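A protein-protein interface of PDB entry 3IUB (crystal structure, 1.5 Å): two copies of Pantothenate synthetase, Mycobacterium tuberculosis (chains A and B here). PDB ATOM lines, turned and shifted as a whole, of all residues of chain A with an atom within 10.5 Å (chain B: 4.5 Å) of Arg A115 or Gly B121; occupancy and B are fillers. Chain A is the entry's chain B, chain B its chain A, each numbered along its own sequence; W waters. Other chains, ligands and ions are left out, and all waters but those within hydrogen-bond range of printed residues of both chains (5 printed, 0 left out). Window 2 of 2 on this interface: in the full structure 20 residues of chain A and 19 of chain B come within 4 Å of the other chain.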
ATOM      1  N   MET A  71     -33.085 -27.496  -1.765  1.00  0.00           N
ATOM      2  CA  MET A  71     -32.681 -27.279  -0.374  1.00  0.00           C
ATOM      3  C   MET A  71     -33.621 -27.911   0.669  1.00  0.00           C
ATOM      4  O   MET A  71     -33.209 -28.151   1.812  1.00  0.00           O
ATOM      5  CB  MET A  71     -32.549 -25.775  -0.123  1.00  0.00           C
ATOM      6  CG  MET A  71     -31.800 -25.390   1.122  1.00  0.00           C
ATOM      7  SD  MET A  71     -31.989 -23.630   1.445  1.00  0.00           S
ATOM      8  CE  MET A  71     -31.516 -23.619   3.174  1.00  0.00           C
ATOM      9  N   MET A 109     -32.852 -18.719  -8.512  1.00  0.00           N
ATOM     10  CA  MET A 109     -33.172 -18.555  -7.099  1.00  0.00           C
ATOM     11  C   MET A 109     -31.918 -18.511  -6.251  1.00  0.00           C
ATOM     12  O   MET A 109     -31.855 -17.794  -5.242  1.00  0.00           O
ATOM     13  CB  MET A 109     -34.122 -19.659  -6.631  1.00  0.00           C
ATOM     14  CG  MET A 109     -35.519 -19.454  -7.179  1.00  0.00           C
ATOM     15  SD  MET A 109     -36.361 -18.017  -6.454  1.00  0.00           S
ATOM     16  CE  MET A 109     -36.799 -18.648  -4.843  1.00  0.00           C
ATOM     17  N   TYR A 110     -30.909 -19.264  -6.673  1.00  0.00           N
ATOM     18  CA  TYR A 110     -29.661 -19.362  -5.924  1.00  0.00           C
ATOM     19  C   TYR A 110     -28.441 -18.989  -6.787  1.00  0.00           C
ATOM     20  O   TYR A 110     -27.562 -19.835  -7.010  1.00  0.00           O
ATOM     21  CB  TYR A 110     -29.523 -20.771  -5.338  1.00  0.00           C
ATOM     22  CG  TYR A 110     -30.598 -21.140  -4.340  1.00  0.00           C
ATOM     23  CD1 TYR A 110     -30.468 -20.786  -2.990  1.00  0.00           C
ATOM     24  CD2 TYR A 110     -31.729 -21.855  -4.733  1.00  0.00           C
ATOM     25  CE1 TYR A 110     -31.447 -21.115  -2.063  1.00  0.00           C
ATOM     26  CE2 TYR A 110     -32.717 -22.199  -3.802  1.00  0.00           C
ATOM     27  CZ  TYR A 110     -32.563 -21.822  -2.473  1.00  0.00           C
ATOM     28  OH  TYR A 110     -33.519 -22.146  -1.533  1.00  0.00           O
ATOM     29  N   PRO A 111     -28.389 -17.734  -7.274  1.00  0.00           N
ATOM     30  CA  PRO A 111     -27.303 -17.346  -8.198  1.00  0.00           C
ATOM     31  C   PRO A 111     -25.924 -17.381  -7.560  1.00  0.00           C
ATOM     32  O   PRO A 111     -24.919 -17.555  -8.263  1.00  0.00           O
ATOM     33  CB  PRO A 111     -27.672 -15.915  -8.607  1.00  0.00           C
ATOM     34  CG  PRO A 111     -28.548 -15.395  -7.461  1.00  0.00           C
ATOM     35  CD  PRO A 111     -29.319 -16.614  -7.012  1.00  0.00           C
ATOM     36  N   ASP A 112     -25.871 -17.233  -6.243  1.00  0.00           N
ATOM     37  CA  ASP A 112     -24.604 -17.321  -5.520  1.00  0.00           C
ATOM     38  C   ASP A 112     -24.466 -18.635  -4.748  1.00  0.00           C
ATOM     39  O   ASP A 112     -23.670 -18.734  -3.809  1.00  0.00           O
ATOM     40  CB  ASP A 112     -24.465 -16.097  -4.601  1.00  0.00           C
ATOM     41  CG  ASP A 112     -24.575 -14.803  -5.372  1.00  0.00           C
ATOM     42  OD1 ASP A 112     -23.602 -14.453  -6.076  1.00  0.00           O
ATOM     43  OD2 ASP A 112     -25.629 -14.132  -5.321  1.00  0.00           O
ATOM     44  N   GLY A 113     -25.262 -19.639  -5.121  1.00  0.00           N
ATOM     45  CA  GLY A 113     -25.311 -20.898  -4.400  1.00  0.00           C
ATOM     46  C   GLY A 113     -25.909 -20.758  -3.005  1.00  0.00           C
ATOM     47  O   GLY A 113     -26.505 -19.718  -2.685  1.00  0.00           O
ATOM     48  N   LEU A 114     -25.764 -21.799  -2.187  1.00  0.00           N
ATOM     49  CA  LEU A 114     -26.241 -21.746  -0.805  1.00  0.00           C
ATOM     50  C   LEU A 114     -25.287 -20.912   0.028  1.00  0.00           C
ATOM     51  O   LEU A 114     -24.096 -21.191   0.109  1.00  0.00           O
ATOM     52  CB  LEU A 114     -26.398 -23.136  -0.190  1.00  0.00           C
ATOM     53  CG  LEU A 114     -27.643 -23.955  -0.532  1.00  0.00           C
ATOM     54  CD1 LEU A 114     -27.625 -25.263   0.228  1.00  0.00           C
ATOM     55  CD2 LEU A 114     -28.917 -23.174  -0.221  1.00  0.00           C
ATOM     56  N   ARG A 115     -25.819 -19.855   0.638  1.00  0.00           N
ATOM     57  CA  ARG A 115     -24.965 -18.944   1.381  1.00  0.00           C
ATOM     58  C   ARG A 115     -25.728 -18.518   2.635  1.00  0.00           C
ATOM     59  O   ARG A 115     -25.747 -19.278   3.605  1.00  0.00           O
ATOM     60  CB  ARG A 115     -24.512 -17.777   0.482  1.00  0.00           C
ATOM     61  CG  ARG A 115     -23.368 -16.980   1.093  1.00  0.00           C
ATOM     62  CD  ARG A 115     -22.697 -16.030   0.094  1.00  0.00           C
ATOM     63  NE  ARG A 115     -23.655 -15.090  -0.498  1.00  0.00           N
ATOM     64  CZ  ARG A 115     -23.357 -14.220  -1.463  1.00  0.00           C
ATOM     65  NH1 ARG A 115     -22.114 -14.138  -1.944  1.00  0.00           N
ATOM     66  NH2 ARG A 115     -24.291 -13.433  -1.957  1.00  0.00           N
ATOM     67  N   THR A 116     -26.372 -17.350   2.620  1.00  0.00           N
ATOM     68  CA  THR A 116     -27.198 -16.945   3.757  1.00  0.00           C
ATOM     69  C   THR A 116     -28.476 -17.770   3.734  1.00  0.00           C
ATOM     70  O   THR A 116     -29.127 -17.882   2.684  1.00  0.00           O
ATOM     71  CB  THR A 116     -27.598 -15.466   3.690  1.00  0.00           C
ATOM     72  OG1 THR A 116     -26.477 -14.667   3.298  1.00  0.00           O
ATOM     73  CG2 THR A 116     -28.117 -14.988   5.049  1.00  0.00           C
ATOM     74  N   THR A 117     -28.847 -18.326   4.883  1.00  0.00           N
ATOM     75  CA  THR A 117     -30.072 -19.110   4.971  1.00  0.00           C
ATOM     76  C   THR A 117     -30.852 -18.783   6.241  1.00  0.00           C
ATOM     77  O   THR A 117     -30.374 -18.046   7.131  1.00  0.00           O
ATOM     78  CB  THR A 117     -29.779 -20.648   4.922  1.00  0.00           C
ATOM     79  OG1 THR A 117     -28.970 -21.018   6.040  1.00  0.00           O
ATOM     80  CG2 THR A 117     -29.102 -21.066   3.598  1.00  0.00           C
ATOM     81  N   VAL A 118     -32.066 -19.329   6.332  1.00  0.00           N
ATOM     82  CA  VAL A 118     -32.886 -19.157   7.528  1.00  0.00           C
ATOM     83  C   VAL A 118     -32.669 -20.367   8.413  1.00  0.00           C
ATOM     84  O   VAL A 118     -32.724 -21.513   7.941  1.00  0.00           O
ATOM     85  CB  VAL A 118     -34.383 -19.065   7.187  1.00  0.00           C
ATOM     86  CG1 VAL A 118     -35.244 -18.957   8.472  1.00  0.00           C
ATOM     87  CG2 VAL A 118     -34.637 -17.923   6.224  1.00  0.00           C
ATOM     88  N   GLN A 119     -32.377 -20.096   9.682  1.00  0.00           N
ATOM     89  CA  GLN A 119     -32.299 -21.133  10.698  1.00  0.00           C
ATOM     90  C   GLN A 119     -33.569 -21.091  11.551  1.00  0.00           C
ATOM     91  O   GLN A 119     -33.768 -20.170  12.342  1.00  0.00           O
ATOM     92  CB  GLN A 119     -31.051 -20.945  11.563  1.00  0.00           C
ATOM     93  CG  GLN A 119     -30.869 -21.986  12.664  1.00  0.00           C
ATOM     94  CD  GLN A 119     -29.516 -21.874  13.358  1.00  0.00           C
ATOM     95  OE1 GLN A 119     -28.473 -21.830  12.713  1.00  0.00           O
ATOM     96  NE2 GLN A 119     -29.537 -21.828  14.681  1.00  0.00           N
ATOM     97  N   ALA A 137     -35.446 -25.635   7.397  1.00  0.00           N
ATOM     98  CA  ALA A 137     -34.495 -24.598   6.986  1.00  0.00           C
ATOM     99  C   ALA A 137     -34.647 -24.302   5.502  1.00  0.00           C
ATOM    100  O   ALA A 137     -34.720 -23.145   5.101  1.00  0.00           O
ATOM    101  CB  ALA A 137     -33.064 -24.992   7.307  1.00  0.00           C
ATOM    102  N   THR A 141     -36.249 -20.838   4.041  1.00  0.00           N
ATOM    103  CA  THR A 141     -35.366 -20.030   3.195  1.00  0.00           C
ATOM    104  C   THR A 141     -36.038 -19.666   1.859  1.00  0.00           C
ATOM    105  O   THR A 141     -36.065 -18.504   1.435  1.00  0.00           O
ATOM    106  CB  THR A 141     -33.997 -20.688   2.975  1.00  0.00           C
ATOM    107  OG1 THR A 141     -33.347 -20.955   4.237  1.00  0.00           O
ATOM    108  CG2 THR A 141     -33.115 -19.810   2.101  1.00  0.00           C
ATOM    109  N   LYS A 145     -37.496 -15.915   0.547  1.00  0.00           N
ATOM    110  CA  LYS A 145     -37.107 -15.365  -0.749  1.00  0.00           C
ATOM    111  C   LYS A 145     -38.320 -15.059  -1.620  1.00  0.00           C
ATOM    112  O   LYS A 145     -38.398 -14.006  -2.196  1.00  0.00           O
ATOM    113  CB  LYS A 145     -36.137 -16.330  -1.459  1.00  0.00           C
ATOM    114  CG  LYS A 145     -34.764 -16.371  -0.752  1.00  0.00           C
ATOM    115  CD  LYS A 145     -33.868 -17.525  -1.196  1.00  0.00           C
ATOM    116  CE  LYS A 145     -33.554 -17.457  -2.704  1.00  0.00           C
ATOM    117  NZ  LYS A 145     -32.769 -16.263  -3.130  1.00  0.00           N
ATOM    118  N   GLN B 119     -28.923 -17.490   9.374  1.00  0.00           N
ATOM    119  CA  GLN B 119     -27.652 -18.208   9.337  1.00  0.00           C
ATOM    120  C   GLN B 119     -26.784 -17.618   8.212  1.00  0.00           C
ATOM    121  O   GLN B 119     -27.070 -17.838   7.029  1.00  0.00           O
ATOM    122  CB  GLN B 119     -27.877 -19.691   9.054  1.00  0.00           C
ATOM    123  CG  GLN B 119     -26.593 -20.478   9.031  1.00  0.00           C
ATOM    124  CD  GLN B 119     -26.438 -21.308  10.263  1.00  0.00           C
ATOM    125  OE1 GLN B 119     -26.934 -22.434  10.323  1.00  0.00           O
ATOM    126  NE2 GLN B 119     -25.771 -20.762  11.270  1.00  0.00           N
ATOM    127  N   PRO B 120     -25.716 -16.867   8.559  1.00  0.00           N
ATOM    128  CA  PRO B 120     -24.877 -16.321   7.505  1.00  0.00           C
ATOM    129  C   PRO B 120     -24.120 -17.428   6.790  1.00  0.00           C
ATOM    130  O   PRO B 120     -24.016 -18.573   7.298  1.00  0.00           O
ATOM    131  CB  PRO B 120     -23.869 -15.432   8.261  1.00  0.00           C
ATOM    132  CG  PRO B 120     -24.392 -15.277   9.651  1.00  0.00           C
ATOM    133  CD  PRO B 120     -25.223 -16.510   9.900  1.00  0.00           C
ATOM    134  N   GLY B 121     -23.572 -17.076   5.629  1.00  0.00           N
ATOM    135  CA  GLY B 121     -22.671 -17.977   4.913  1.00  0.00           C
ATOM    136  C   GLY B 121     -21.331 -18.108   5.635  1.00  0.00           C
ATOM    137  O   GLY B 121     -21.130 -17.543   6.716  1.00  0.00           O
ATOM    138  N   PRO B 122     -20.398 -18.873   5.036  1.00  0.00           N
ATOM    139  CA  PRO B 122     -19.114 -19.245   5.637  1.00  0.00           C
ATOM    140  C   PRO B 122     -18.243 -18.057   6.048  1.00  0.00           C
ATOM    141  O   PRO B 122     -17.422 -18.211   6.955  1.00  0.00           O
ATOM    142  CB  PRO B 122     -18.427 -20.062   4.533  1.00  0.00           C
ATOM    143  CG  PRO B 122     -19.526 -20.533   3.662  1.00  0.00           C
ATOM    144  CD  PRO B 122     -20.586 -19.473   3.703  1.00  0.00           C
ATOM    145  N   LEU B 123     -18.427 -16.897   5.411  1.00  0.00           N
ATOM    146  CA  LEU B 123     -17.650 -15.702   5.799  1.00  0.00           C
ATOM    147  C   LEU B 123     -17.835 -15.354   7.275  1.00  0.00           C
ATOM    148  O   LEU B 123     -16.941 -14.768   7.898  1.00  0.00           O
ATOM    149  CB  LEU B 123     -17.982 -14.503   4.898  1.00  0.00           C
ATOM    150  CG  LEU B 123     -17.379 -13.136   5.271  1.00  0.00           C
ATOM    151  CD1 LEU B 123     -15.842 -13.135   5.357  1.00  0.00           C
ATOM    152  CD2 LEU B 123     -17.846 -12.102   4.280  1.00  0.00           C
ATOM    153  N   ALA B 124     -18.976 -15.730   7.853  1.00  0.00           N
ATOM    154  CA  ALA B 124     -19.257 -15.383   9.244  1.00  0.00           C
ATOM    155  C   ALA B 124     -18.361 -16.121  10.228  1.00  0.00           C
ATOM    156  O   ALA B 124     -18.301 -15.741  11.390  1.00  0.00           O
ATOM    157  CB  ALA B 124     -20.692 -15.670   9.557  1.00  0.00           C
ATOM    158  N   GLN B 170     -24.483  -9.671   1.384  1.00  0.00           N
ATOM    159  CA  GLN B 170     -24.847 -11.075   1.158  1.00  0.00           C
ATOM    160  C   GLN B 170     -26.298 -11.302   1.589  1.00  0.00           C
ATOM    161  O   GLN B 170     -27.089 -11.883   0.851  1.00  0.00           O
ATOM    162  CB  GLN B 170     -23.899 -12.015   1.896  1.00  0.00           C
ATOM    163  CG  GLN B 170     -22.494 -11.993   1.287  1.00  0.00           C
ATOM    164  CD  GLN B 170     -21.578 -13.052   1.840  1.00  0.00           C
ATOM    165  OE1 GLN B 170     -21.946 -13.806   2.737  1.00  0.00           O
ATOM    166  NE2 GLN B 170     -20.365 -13.128   1.281  1.00  0.00           N
ATOM    167  N   ALA B 173     -28.651  -9.731  -1.056  1.00  0.00           N
ATOM    168  CA  ALA B 173     -28.684 -10.511  -2.286  1.00  0.00           C
ATOM    169  C   ALA B 173     -29.388 -11.844  -2.082  1.00  0.00           C
ATOM    170  O   ALA B 173     -30.255 -12.250  -2.892  1.00  0.00           O
ATOM    171  CB  ALA B 173     -27.266 -10.726  -2.795  1.00  0.00           C
ATOM    172  N   ASP B 174     -29.003 -12.544  -1.016  1.00  0.00           N
ATOM    173  CA  ASP B 174     -29.442 -13.921  -0.802  1.00  0.00           C
ATOM    174  C   ASP B 174     -30.917 -14.046  -0.450  1.00  0.00           C
ATOM    175  O   ASP B 174     -31.548 -15.070  -0.754  1.00  0.00           O
ATOM    176  CB  ASP B 174     -28.597 -14.588   0.280  1.00  0.00           C
ATOM    177  CG  ASP B 174     -27.142 -14.749  -0.141  1.00  0.00           C
ATOM    178  OD1 ASP B 174     -26.832 -14.508  -1.325  1.00  0.00           O
ATOM    179  OD2 ASP B 174     -26.308 -15.087   0.718  1.00  0.00           O
HETATM  180  O   HOH W   1     -24.027 -14.485   4.609  1.00  0.00           O
HETATM  181  O   HOH W   2     -30.456 -14.654  -4.333  1.00  0.00           O
HETATM  182  O   HOH W   3     -25.602 -22.715  13.540  1.00  0.00           O
HETATM  183  O   HOH W   4     -27.693 -14.928  -3.827  1.00  0.00           O
HETATM  184  O   HOH W   5     -26.345 -20.763   5.784  1.00  0.00           O
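Arg A115 touches just these residues of chain B: Gln B119 (3.9 Å), Gly B121 (3.6 Å), Gln B170 (3.5 Å) and Asp B174 (2.8 Å).
Printed residues of chain B within 4 Å of Thr A117: Gln B119 (2.7 Å).
Printed residues of chain B within 4 Å of Gln A119: Gln B119.
Of the printed residues of chain A, Gln B119 touches Arg A115 (3.9 Å), Thr A116 (3.4 Å), Thr A117 (2.7 Å) and Gln A119 (2.9 Å).
Of chain A, only Arg A115 comes within 4 Å of Gly B121.
No residue of chain A comes within 4 Å of Pro B122.
Gln B170 touches two residues of chain A.
No residue of chain A comes within 4 Å of Ala B173.
Of the printed residues of chain A, Asp B174 touches Arg A115, Thr A116 and Lys A145.
The nearest residue of chain B that does not touch Arg A115 is Pro B120 (4.03 Å).
The nearest residue of chain A that does not touch Gly B121 is Thr A116 (4.1 Å).
The nearest printed residue of chain B that does not touch Lys A145 is Ala B173 (4.7 Å).
Water W5 lies within hydrogen-bond range of OG1 of Thr A117 (2.6 Å), O of Arg A115 (2.7 Å) and O of Gln B119 (3.3 Å).
Water W4 bridges the side-chain carboxylate of Asp A112 (2.7 Å) and the side-chain carboxylate of Asp B174 (2.7 Å).
Water W1 lies within hydrogen-bond range of the side-chain hydroxyl of Thr A116 (2.8 Å), the backbone NH of Gly B121 (2.8 Å) and the side-chain amide oxygen of Gln B170 (2.9 Å).
Water W2 lies within hydrogen-bond range of the backbone carbonyl oxygen (O) of Ala B173 (2.8 Å) and the side-chain amino group (NZ) of Lys A145 (3.1 Å).
Water W3 lies within hydrogen-bond range of NE2 of Gln B119 (3.0 Å) and OE1 of Gln A119 (3.1 Å).
Gln B119 touches its own counterpart, Gln A119.
Of the 10 pairs that touch across the chains among the printed residues, 1 has its exchanged pair printed and touching as well.
Of the 9 printed residues of chain B, 4 touch a printed residue of chain A.
Among the printed residues, 10 pairs touch across the chains.
O of Met A109 is in hydrogen-bond range of NZ of Lys A145, at 2.8 Å.
OD2 of Asp A112 is in salt-bridge range of NH2 of Arg A115 (3.7 Å).
N of Gln B119 sits at hydrogen-bond distance from O of Thr A117 (2.7 Å).
The side-chain amide oxygen (OE1) of Gln B119 lies close to the side-chain amide oxygen (OE1) of Gln A119 (2.9 Å).
OD1 of Asp B174 is in salt-bridge range of NH2 of Arg A115 (2.8 Å).
The side-chain hydroxyl (OG1) of Thr A116 lies within hydrogen-bond range of the side-chain carboxylate (OD2) of Asp B174 (2.6 Å).
The side-chain amino group (NZ) of Lys A145 lies within hydrogen-bond range of the backbone carbonyl oxygen (O) of Asp B174.
Among the printed residues, pairs that only touch across the chains: Arg A115 with Gln B119 (3.9 Å), Arg A115 with Gly B121 (3.6 Å), Arg A115 with Gln B170 (3.5 Å), Thr A116 with Gln B119 (3.4 Å) and Thr A116 with Gln B170 (3.8 Å).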
